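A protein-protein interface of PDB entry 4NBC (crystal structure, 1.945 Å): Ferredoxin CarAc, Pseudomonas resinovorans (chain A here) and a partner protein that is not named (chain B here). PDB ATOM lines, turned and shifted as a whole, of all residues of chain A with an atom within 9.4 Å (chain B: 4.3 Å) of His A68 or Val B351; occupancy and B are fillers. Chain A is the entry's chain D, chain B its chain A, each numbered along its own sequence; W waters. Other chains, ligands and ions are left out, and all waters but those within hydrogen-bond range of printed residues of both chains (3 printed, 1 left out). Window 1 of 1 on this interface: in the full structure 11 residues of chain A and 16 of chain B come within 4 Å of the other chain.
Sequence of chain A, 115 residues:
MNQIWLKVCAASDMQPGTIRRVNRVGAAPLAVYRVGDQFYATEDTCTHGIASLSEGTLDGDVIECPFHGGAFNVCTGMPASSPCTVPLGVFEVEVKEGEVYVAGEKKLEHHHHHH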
ATOM      1  N   CYS A  46      13.047   9.986 -19.141  1.00  0.00           N
ATOM      2  CA  CYS A  46      12.609  11.318 -19.537  1.00  0.00           C
ATOM      3  C   CYS A  46      11.096  11.269 -19.744  1.00  0.00           C
ATOM      4  O   CYS A  46      10.585  10.328 -20.350  1.00  0.00           O
ATOM      5  CB  CYS A  46      13.298  11.731 -20.836  1.00  0.00           C
ATOM      6  SG  CYS A  46      12.879  13.391 -21.367  1.00  0.00           S
ATOM      7  N   THR A  47      10.387  12.277 -19.241  1.00  0.00           N
ATOM      8  CA  THR A  47       8.929  12.325 -19.360  1.00  0.00           C
ATOM      9  C   THR A  47       8.447  12.572 -20.788  1.00  0.00           C
ATOM     10  O   THR A  47       7.261  12.411 -21.089  1.00  0.00           O
ATOM     11  CB  THR A  47       8.317  13.422 -18.446  1.00  0.00           C
ATOM     12  OG1 THR A  47       8.771  14.713 -18.867  1.00  0.00           O
ATOM     13  CG2 THR A  47       8.727  13.202 -16.994  1.00  0.00           C
ATOM     14  N   HIS A  48       9.365  12.953 -21.667  1.00  0.00           N
ATOM     15  CA  HIS A  48       9.012  13.223 -23.058  1.00  0.00           C
ATOM     16  C   HIS A  48       9.114  11.977 -23.941  1.00  0.00           C
ATOM     17  O   HIS A  48       8.702  11.996 -25.101  1.00  0.00           O
ATOM     18  CB  HIS A  48       9.916  14.334 -23.608  1.00  0.00           C
ATOM     19  CG  HIS A  48       9.699  14.640 -25.059  1.00  0.00           C
ATOM     20  ND1 HIS A  48      10.598  14.279 -26.038  1.00  0.00           N
ATOM     21  CD2 HIS A  48       8.695  15.293 -25.695  1.00  0.00           C
ATOM     22  CE1 HIS A  48      10.162  14.696 -27.214  1.00  0.00           C
ATOM     23  NE2 HIS A  48       9.008  15.314 -27.034  1.00  0.00           N
ATOM     24  N   GLY A  49       9.654  10.891 -23.396  1.00  0.00           N
ATOM     25  CA  GLY A  49       9.792   9.680 -24.186  1.00  0.00           C
ATOM     26  C   GLY A  49      10.219   8.459 -23.401  1.00  0.00           C
ATOM     27  O   GLY A  49       9.584   8.103 -22.409  1.00  0.00           O
ATOM     28  N   ILE A  50      11.288   7.810 -23.851  1.00  0.00           N
ATOM     29  CA  ILE A  50      11.800   6.611 -23.195  1.00  0.00           C
ATOM     30  C   ILE A  50      13.314   6.667 -22.978  1.00  0.00           C
ATOM     31  O   ILE A  50      13.960   5.637 -22.764  1.00  0.00           O
ATOM     32  CB  ILE A  50      11.471   5.343 -24.017  1.00  0.00           C
ATOM     33  CG1 ILE A  50      12.073   5.452 -25.421  1.00  0.00           C
ATOM     34  CG2 ILE A  50       9.967   5.156 -24.092  1.00  0.00           C
ATOM     35  CD1 ILE A  50      11.825   4.236 -26.291  1.00  0.00           C
ATOM     36  N   ALA A  51      13.876   7.870 -23.036  1.00  0.00           N
ATOM     37  CA  ALA A  51      15.312   8.047 -22.843  1.00  0.00           C
ATOM     38  C   ALA A  51      15.716   7.947 -21.372  1.00  0.00           C
ATOM     39  O   ALA A  51      14.915   8.216 -20.472  1.00  0.00           O
ATOM     40  CB  ALA A  51      15.741   9.395 -23.395  1.00  0.00           C
ATOM     41  N   SER A  52      16.967   7.555 -21.142  1.00  0.00           N
ATOM     42  CA  SER A  52      17.514   7.446 -19.795  1.00  0.00           C
ATOM     43  C   SER A  52      18.312   8.713 -19.517  1.00  0.00           C
ATOM     44  O   SER A  52      19.362   8.938 -20.116  1.00  0.00           O
ATOM     45  CB  SER A  52      18.436   6.226 -19.683  1.00  0.00           C
ATOM     46  OG  SER A  52      19.154   6.252 -18.456  1.00  0.00           O
ATOM     47  N   LEU A  53      17.806   9.542 -18.611  1.00  0.00           N
ATOM     48  CA  LEU A  53      18.465  10.799 -18.268  1.00  0.00           C
ATOM     49  C   LEU A  53      19.871  10.612 -17.703  1.00  0.00           C
ATOM     50  O   LEU A  53      20.698  11.520 -17.779  1.00  0.00           O
ATOM     51  CB  LEU A  53      17.611  11.586 -17.270  1.00  0.00           C
ATOM     52  CG  LEU A  53      16.279  12.104 -17.821  1.00  0.00           C
ATOM     53  CD1 LEU A  53      15.463  12.717 -16.695  1.00  0.00           C
ATOM     54  CD2 LEU A  53      16.547  13.132 -18.925  1.00  0.00           C
ATOM     55  N   GLY A  56      22.427  11.316 -19.998  1.00  0.00           N
ATOM     56  CA  GLY A  56      22.406  12.681 -20.491  1.00  0.00           C
ATOM     57  C   GLY A  56      23.577  13.522 -20.010  1.00  0.00           C
ATOM     58  O   GLY A  56      24.591  12.995 -19.565  1.00  0.00           O
ATOM     59  N   GLU A  64      20.213  17.445 -19.152  1.00  0.00           N
ATOM     60  CA  GLU A  64      19.768  17.471 -20.545  1.00  0.00           C
ATOM     61  C   GLU A  64      19.575  16.055 -21.070  1.00  0.00           C
ATOM     62  O   GLU A  64      20.477  15.222 -20.961  1.00  0.00           O
ATOM     63  CB  GLU A  64      20.797  18.192 -21.419  1.00  0.00           C
ATOM     64  CG  GLU A  64      20.424  18.244 -22.895  1.00  0.00           C
ATOM     65  CD  GLU A  64      21.578  18.692 -23.780  1.00  0.00           C
ATOM     66  OE1 GLU A  64      22.554  17.923 -23.934  1.00  0.00           O
ATOM     67  OE2 GLU A  64      21.512  19.814 -24.320  1.00  0.00           O
ATOM     68  N   CYS A  65      18.402  15.788 -21.638  1.00  0.00           N
ATOM     69  CA  CYS A  65      18.091  14.465 -22.180  1.00  0.00           C
ATOM     70  C   CYS A  65      18.892  14.191 -23.452  1.00  0.00           C
ATOM     71  O   CYS A  65      18.994  15.049 -24.323  1.00  0.00           O
ATOM     72  CB  CYS A  65      16.599  14.350 -22.491  1.00  0.00           C
ATOM     73  SG  CYS A  65      16.159  12.747 -23.190  1.00  0.00           S
ATOM     74  N   PRO A  66      19.458  12.980 -23.579  1.00  0.00           N
ATOM     75  CA  PRO A  66      20.257  12.590 -24.745  1.00  0.00           C
ATOM     76  C   PRO A  66      19.483  12.411 -26.055  1.00  0.00           C
ATOM     77  O   PRO A  66      20.063  12.492 -27.140  1.00  0.00           O
ATOM     78  CB  PRO A  66      20.914  11.291 -24.286  1.00  0.00           C
ATOM     79  CG  PRO A  66      19.874  10.696 -23.400  1.00  0.00           C
ATOM     80  CD  PRO A  66      19.411  11.888 -22.592  1.00  0.00           C
ATOM     81  N   PHE A  67      18.179  12.179 -25.955  1.00  0.00           N
ATOM     82  CA  PHE A  67      17.356  11.967 -27.145  1.00  0.00           C
ATOM     83  C   PHE A  67      17.050  13.203 -27.981  1.00  0.00           C
ATOM     84  O   PHE A  67      17.425  13.269 -29.152  1.00  0.00           O
ATOM     85  CB  PHE A  67      16.029  11.302 -26.755  1.00  0.00           C
ATOM     86  CG  PHE A  67      16.093   9.805 -26.678  1.00  0.00           C
ATOM     87  CD1 PHE A  67      17.289   9.151 -26.389  1.00  0.00           C
ATOM     88  CD2 PHE A  67      14.943   9.045 -26.860  1.00  0.00           C
ATOM     89  CE1 PHE A  67      17.336   7.756 -26.281  1.00  0.00           C
ATOM     90  CE2 PHE A  67      14.977   7.652 -26.754  1.00  0.00           C
ATOM     91  CZ  PHE A  67      16.174   7.007 -26.464  1.00  0.00           C
ATOM     92  N   HIS A  68      16.371  14.177 -27.384  1.00  0.00           N
ATOM     93  CA  HIS A  68      15.983  15.368 -28.125  1.00  0.00           C
ATOM     94  C   HIS A  68      16.483  16.692 -27.552  1.00  0.00           C
ATOM     95  O   HIS A  68      16.150  17.757 -28.064  1.00  0.00           O
ATOM     96  CB  HIS A  68      14.458  15.396 -28.248  1.00  0.00           C
ATOM     97  CG  HIS A  68      13.868  14.099 -28.716  1.00  0.00           C
ATOM     98  ND1 HIS A  68      13.085  13.303 -27.909  1.00  0.00           N
ATOM     99  CD2 HIS A  68      13.966  13.450 -29.901  1.00  0.00           C
ATOM    100  CE1 HIS A  68      12.725  12.220 -28.575  1.00  0.00           C
ATOM    101  NE2 HIS A  68      13.246  12.285 -29.788  1.00  0.00           N
ATOM    102  N   GLY A  69      17.281  16.635 -26.494  1.00  0.00           N
ATOM    103  CA  GLY A  69      17.801  17.865 -25.916  1.00  0.00           C
ATOM    104  C   GLY A  69      16.867  18.569 -24.945  1.00  0.00           C
ATOM    105  O   GLY A  69      17.096  19.729 -24.595  1.00  0.00           O
ATOM    106  N   GLY A  70      15.799  17.892 -24.532  1.00  0.00           N
ATOM    107  CA  GLY A  70      14.894  18.481 -23.560  1.00  0.00           C
ATOM    108  C   GLY A  70      15.666  18.495 -22.250  1.00  0.00           C
ATOM    109  O   GLY A  70      16.677  17.800 -22.135  1.00  0.00           O
ATOM    110  N   ALA A  71      15.219  19.264 -21.262  1.00  0.00           N
ATOM    111  CA  ALA A  71      15.944  19.320 -19.997  1.00  0.00           C
ATOM    112  C   ALA A  71      15.050  19.579 -18.789  1.00  0.00           C
ATOM    113  O   ALA A  71      13.938  20.084 -18.918  1.00  0.00           O
ATOM    114  CB  ALA A  71      17.045  20.389 -20.077  1.00  0.00           C
ATOM    115  N   SER A  81      14.011  22.932 -20.631  1.00  0.00           N
ATOM    116  CA  SER A  81      14.138  23.144 -22.068  1.00  0.00           C
ATOM    117  C   SER A  81      13.106  22.332 -22.841  1.00  0.00           C
ATOM    118  O   SER A  81      12.725  21.237 -22.427  1.00  0.00           O
ATOM    119  CB  SER A  81      15.537  22.738 -22.557  1.00  0.00           C
ATOM    120  OG  SER A  81      16.557  23.537 -21.986  1.00  0.00           O
ATOM    121  N   SER A  82      12.662  22.874 -23.968  1.00  0.00           N
ATOM    122  CA  SER A  82      11.711  22.178 -24.826  1.00  0.00           C
ATOM    123  C   SER A  82      12.488  20.975 -25.368  1.00  0.00           C
ATOM    124  O   SER A  82      13.718  20.987 -25.370  1.00  0.00           O
ATOM    125  CB  SER A  82      11.287  23.090 -25.979  1.00  0.00           C
ATOM    126  OG  SER A  82      12.425  23.535 -26.704  1.00  0.00           O
ATOM    127  N   PRO A  83      11.791  19.929 -25.846  1.00  0.00           N
ATOM    128  CA  PRO A  83      10.336  19.749 -25.940  1.00  0.00           C
ATOM    129  C   PRO A  83       9.651  19.260 -24.657  1.00  0.00           C
ATOM    130  O   PRO A  83       8.436  19.068 -24.638  1.00  0.00           O
ATOM    131  CB  PRO A  83      10.196  18.741 -27.075  1.00  0.00           C
ATOM    132  CG  PRO A  83      11.369  17.834 -26.829  1.00  0.00           C
ATOM    133  CD  PRO A  83      12.497  18.820 -26.521  1.00  0.00           C
ATOM    134  N   CYS A  84      10.414  19.057 -23.588  1.00  0.00           N
ATOM    135  CA  CYS A  84       9.825  18.576 -22.337  1.00  0.00           C
ATOM    136  C   CYS A  84       8.786  19.536 -21.753  1.00  0.00           C
ATOM    137  O   CYS A  84       8.979  20.751 -21.761  1.00  0.00           O
ATOM    138  CB  CYS A  84      10.924  18.315 -21.311  1.00  0.00           C
ATOM    139  SG  CYS A  84      12.059  17.003 -21.815  1.00  0.00           S
ATOM    140  N   ILE B   8      19.357  21.419 -34.759  1.00  0.00           N
ATOM    141  CA  ILE B   8      18.590  20.198 -34.580  1.00  0.00           C
ATOM    142  C   ILE B   8      19.542  19.027 -34.358  1.00  0.00           C
ATOM    143  O   ILE B   8      19.352  18.230 -33.442  1.00  0.00           O
ATOM    144  CB  ILE B   8      17.697  19.914 -35.808  1.00  0.00           C
ATOM    145  CG1 ILE B   8      16.653  21.031 -35.954  1.00  0.00           C
ATOM    146  CG2 ILE B   8      17.029  18.552 -35.660  1.00  0.00           C
ATOM    147  CD1 ILE B   8      15.714  20.857 -37.141  1.00  0.00           C
ATOM    148  N   ARG B  11      20.763  18.697 -30.900  1.00  0.00           N
ATOM    149  CA  ARG B  11      19.800  18.123 -29.966  1.00  0.00           C
ATOM    150  C   ARG B  11      19.684  16.601 -29.974  1.00  0.00           C
ATOM    151  O   ARG B  11      19.482  15.988 -28.926  1.00  0.00           O
ATOM    152  CB  ARG B  11      18.414  18.715 -30.222  1.00  0.00           C
ATOM    153  CG  ARG B  11      18.160  20.053 -29.550  1.00  0.00           C
ATOM    154  CD  ARG B  11      16.843  20.644 -30.016  1.00  0.00           C
ATOM    155  NE  ARG B  11      16.433  21.781 -29.201  1.00  0.00           N
ATOM    156  CZ  ARG B  11      15.863  21.676 -28.003  1.00  0.00           C
ATOM    157  NH1 ARG B  11      15.625  20.481 -27.476  1.00  0.00           N
ATOM    158  NH2 ARG B  11      15.539  22.771 -27.327  1.00  0.00           N
ATOM    159  N   LYS B 348      11.674  18.958 -37.692  1.00  0.00           N
ATOM    160  CA  LYS B 348      11.335  19.171 -36.286  1.00  0.00           C
ATOM    161  C   LYS B 348      10.736  17.930 -35.615  1.00  0.00           C
ATOM    162  O   LYS B 348      10.796  17.793 -34.395  1.00  0.00           O
ATOM    163  CB  LYS B 348      10.380  20.365 -36.131  1.00  0.00           C
ATOM    164  CG  LYS B 348      10.957  21.707 -36.609  1.00  0.00           C
ATOM    165  CD  LYS B 348      12.253  22.056 -35.887  1.00  0.00           C
ATOM    166  CE  LYS B 348      12.864  23.363 -36.393  1.00  0.00           C
ATOM    167  NZ  LYS B 348      12.027  24.563 -36.115  1.00  0.00           N
ATOM    168  N   GLY B 349      10.162  17.028 -36.402  1.00  0.00           N
ATOM    169  CA  GLY B 349       9.595  15.820 -35.821  1.00  0.00           C
ATOM    170  C   GLY B 349      10.641  14.985 -35.089  1.00  0.00           C
ATOM    171  O   GLY B 349      10.316  14.255 -34.151  1.00  0.00           O
ATOM    172  N   TRP B 350      11.898  15.089 -35.517  1.00  0.00           N
ATOM    173  CA  TRP B 350      12.989  14.335 -34.898  1.00  0.00           C
ATOM    174  C   TRP B 350      13.271  14.845 -33.487  1.00  0.00           C
ATOM    175  O   TRP B 350      14.016  14.232 -32.726  1.00  0.00           O
ATOM    176  CB  TRP B 350      14.264  14.441 -35.749  1.00  0.00           C
ATOM    177  CG  TRP B 350      14.103  13.924 -37.144  1.00  0.00           C
ATOM    178  CD1 TRP B 350      14.071  14.663 -38.293  1.00  0.00           C
ATOM    179  CD2 TRP B 350      13.952  12.557 -37.543  1.00  0.00           C
ATOM    180  NE1 TRP B 350      13.914  13.841 -39.384  1.00  0.00           N
ATOM    181  CE2 TRP B 350      13.837  12.543 -38.953  1.00  0.00           C
ATOM    182  CE3 TRP B 350      13.901  11.338 -36.847  1.00  0.00           C
ATOM    183  CZ2 TRP B 350      13.673  11.359 -39.683  1.00  0.00           C
ATOM    184  CZ3 TRP B 350      13.738  10.160 -37.571  1.00  0.00           C
ATOM    185  CH2 TRP B 350      13.626  10.181 -38.979  1.00  0.00           C
ATOM    186  N   VAL B 351      12.666  15.973 -33.141  1.00  0.00           N
ATOM    187  CA  VAL B 351      12.838  16.554 -31.818  1.00  0.00           C
ATOM    188  C   VAL B 351      11.539  16.467 -31.013  1.00  0.00           C
ATOM    189  O   VAL B 351      11.552  16.145 -29.823  1.00  0.00           O
ATOM    190  CB  VAL B 351      13.244  18.046 -31.916  1.00  0.00           C
ATOM    191  CG1 VAL B 351      13.228  18.688 -30.535  1.00  0.00           C
ATOM    192  CG2 VAL B 351      14.623  18.171 -32.545  1.00  0.00           C
ATOM    193  N   ASN B 352      10.413  16.727 -31.674  1.00  0.00           N
ATOM    194  CA  ASN B 352       9.122  16.745 -30.996  1.00  0.00           C
ATOM    195  C   ASN B 352       8.351  15.439 -30.805  1.00  0.00           C
ATOM    196  O   ASN B 352       7.391  15.399 -30.032  1.00  0.00           O
ATOM    197  CB  ASN B 352       8.230  17.793 -31.665  1.00  0.00           C
ATOM    198  CG  ASN B 352       8.812  19.189 -31.560  1.00  0.00           C
ATOM    199  OD1 ASN B 352       9.222  19.610 -30.486  1.00  0.00           O
ATOM    200  ND2 ASN B 352       8.850  19.910 -32.674  1.00  0.00           N
ATOM    201  N   GLU B 353       8.767  14.378 -31.491  1.00  0.00           N
ATOM    202  CA  GLU B 353       8.115  13.076 -31.365  1.00  0.00           C
ATOM    203  C   GLU B 353       8.070  12.629 -29.894  1.00  0.00           C
ATOM    204  O   GLU B 353       9.024  12.851 -29.149  1.00  0.00           O
ATOM    205  CB  GLU B 353       8.905  12.035 -32.176  1.00  0.00           C
ATOM    206  CG  GLU B 353      10.396  12.010 -31.802  1.00  0.00           C
ATOM    207  CD  GLU B 353      11.235  11.018 -32.599  1.00  0.00           C
ATOM    208  OE1 GLU B 353      10.807  10.597 -33.697  1.00  0.00           O
ATOM    209  OE2 GLU B 353      12.346  10.678 -32.127  1.00  0.00           O
HETATM  210  O   HOH W   1      10.050  11.064 -27.381  1.00  0.00           O
HETATM  211  O   HOH W   2      12.837  22.031 -28.818  1.00  0.00           O
HETATM  212  O   HOH W   3       6.847  17.395 -27.991  1.00  0.00           O
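Water W2 lies within hydrogen-bond range of OG of Ser A82 (2.6 Å) and NH2 of Arg B11 (3.2 Å).
Water W1 bridges O of Glu B353 (2.7 Å) and O of His A48 (2.8 Å).
Water W3 bridges O of Asn B352 and NE2 of His A48.
The backbone NH (N) of Phe A67 sits close to the side-chain sulfur (SG) of Cys A65, 3.5 Å away.
The side-chain amide nitrogen of Asn B352 is in hydrogen-bond range of the backbone carbonyl oxygen of Lys B348.
The backbone NH (N) of His A48 lies close to the side-chain sulfur (SG) of Cys A46 (3.6 Å).
N of Cys A65 is in hydrogen-bond range of O of Gly A70, at 2.7 Å.
His A68 touches just these residues of chain B: Arg B11 (2.8 Å), Trp B350 (2.9 Å), Val B351 (3.3 Å) and Glu B353 (3.0 Å).
Of chain A, only His A48, His A68 and Pro A83 come within 4 Å of Val B351.
No residue of chain A comes within 4 Å of Gly B349.
Asn B352 touches just these residues of chain A: His A48 (3.4 Å) and Pro A83 (3.7 Å).
Glu B353 touches just these residues of chain A: His A48 and His A68.
Printed residues of chain B within 4 Å of Pro A83: Arg B11, Val B351 and Asn B352.
Of the printed residues of chain B, Gly A70 touches Arg B11.
Printed residues of chain B within 4 Å of Ser A82: Arg B11.
Printed residues of chain A within 4 Å of Trp B350: His A68 (2.9 Å).
Thr A47 touches none of the printed residues of chain B.
Gly A56 touches none of the printed residues of chain B.
The nearest printed residue of chain B that does not touch His A68 is Asn B352 (5.1 Å).
O of Val B351 touches CE1 of His A48 (3.3 Å).
O of Pro A66 touches O of Arg B11 (3.97 Å).
His A68 touches Trp B350 (CD2 to O, 2.9 Å).
Val B351 touches His A68 (O to CG, 3.3 Å).
Arg B11 touches Gly A70.
Pro A83 touches Arg B11 (CD to NH1, 3.7 Å).
CG of Pro A83 touches O of Val B351 (3.4 Å).
Pro A83 touches Asn B352 (CB to OD1, 3.7 Å).
The guanidinium group (NH1) of Arg B11 is in hydrogen-bond range of the backbone carbonyl oxygen (O) of Ser A82 (2.9 Å).
The backbone carbonyl oxygen of Asn B352 is in hydrogen-bond range of a ring nitrogen (NE2) of His A48.
O of Phe A67 lies close to O of Arg B11 (3.4 Å).
NH1 of Arg B11 lies within hydrogen-bond range of O of Gly A69 (3.3 Å).
The side-chain carboxylate (OE2) of Glu B353 lies within hydrogen-bond range of a ring nitrogen (NE2) of His A68, at 3.0 Å.
The backbone carbonyl oxygen of His A68 sits at hydrogen-bond distance from the guanidinium group of Arg B11, at 2.8 Å.
A ring nitrogen (NE2) of His A48 sits close to the backbone carbonyl oxygen (O) of Glu B353, at 3.2 Å.
Of the 8 printed residues of chain B, 5 touch a printed residue of chain A.
Printed residues of chain B that touch a printed residue of chain A: Arg B11, Trp B350, Val B351, Asn B352 and Glu B353.
Hydrophobic or aromatic side chains of chain B within 4 Å of the printed part of chain A: Val B351.
Hydrophobic or aromatic side chains of chain A that line the printed part of chain B: His A48, His A68 and Pro A83.
Among the printed residues, 15 pairs touch across the chains.
Among the printed residues, no Asp or Glu carboxylate lies within 4 Å of a Lys or Arg side-chain nitrogen of the other chain.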
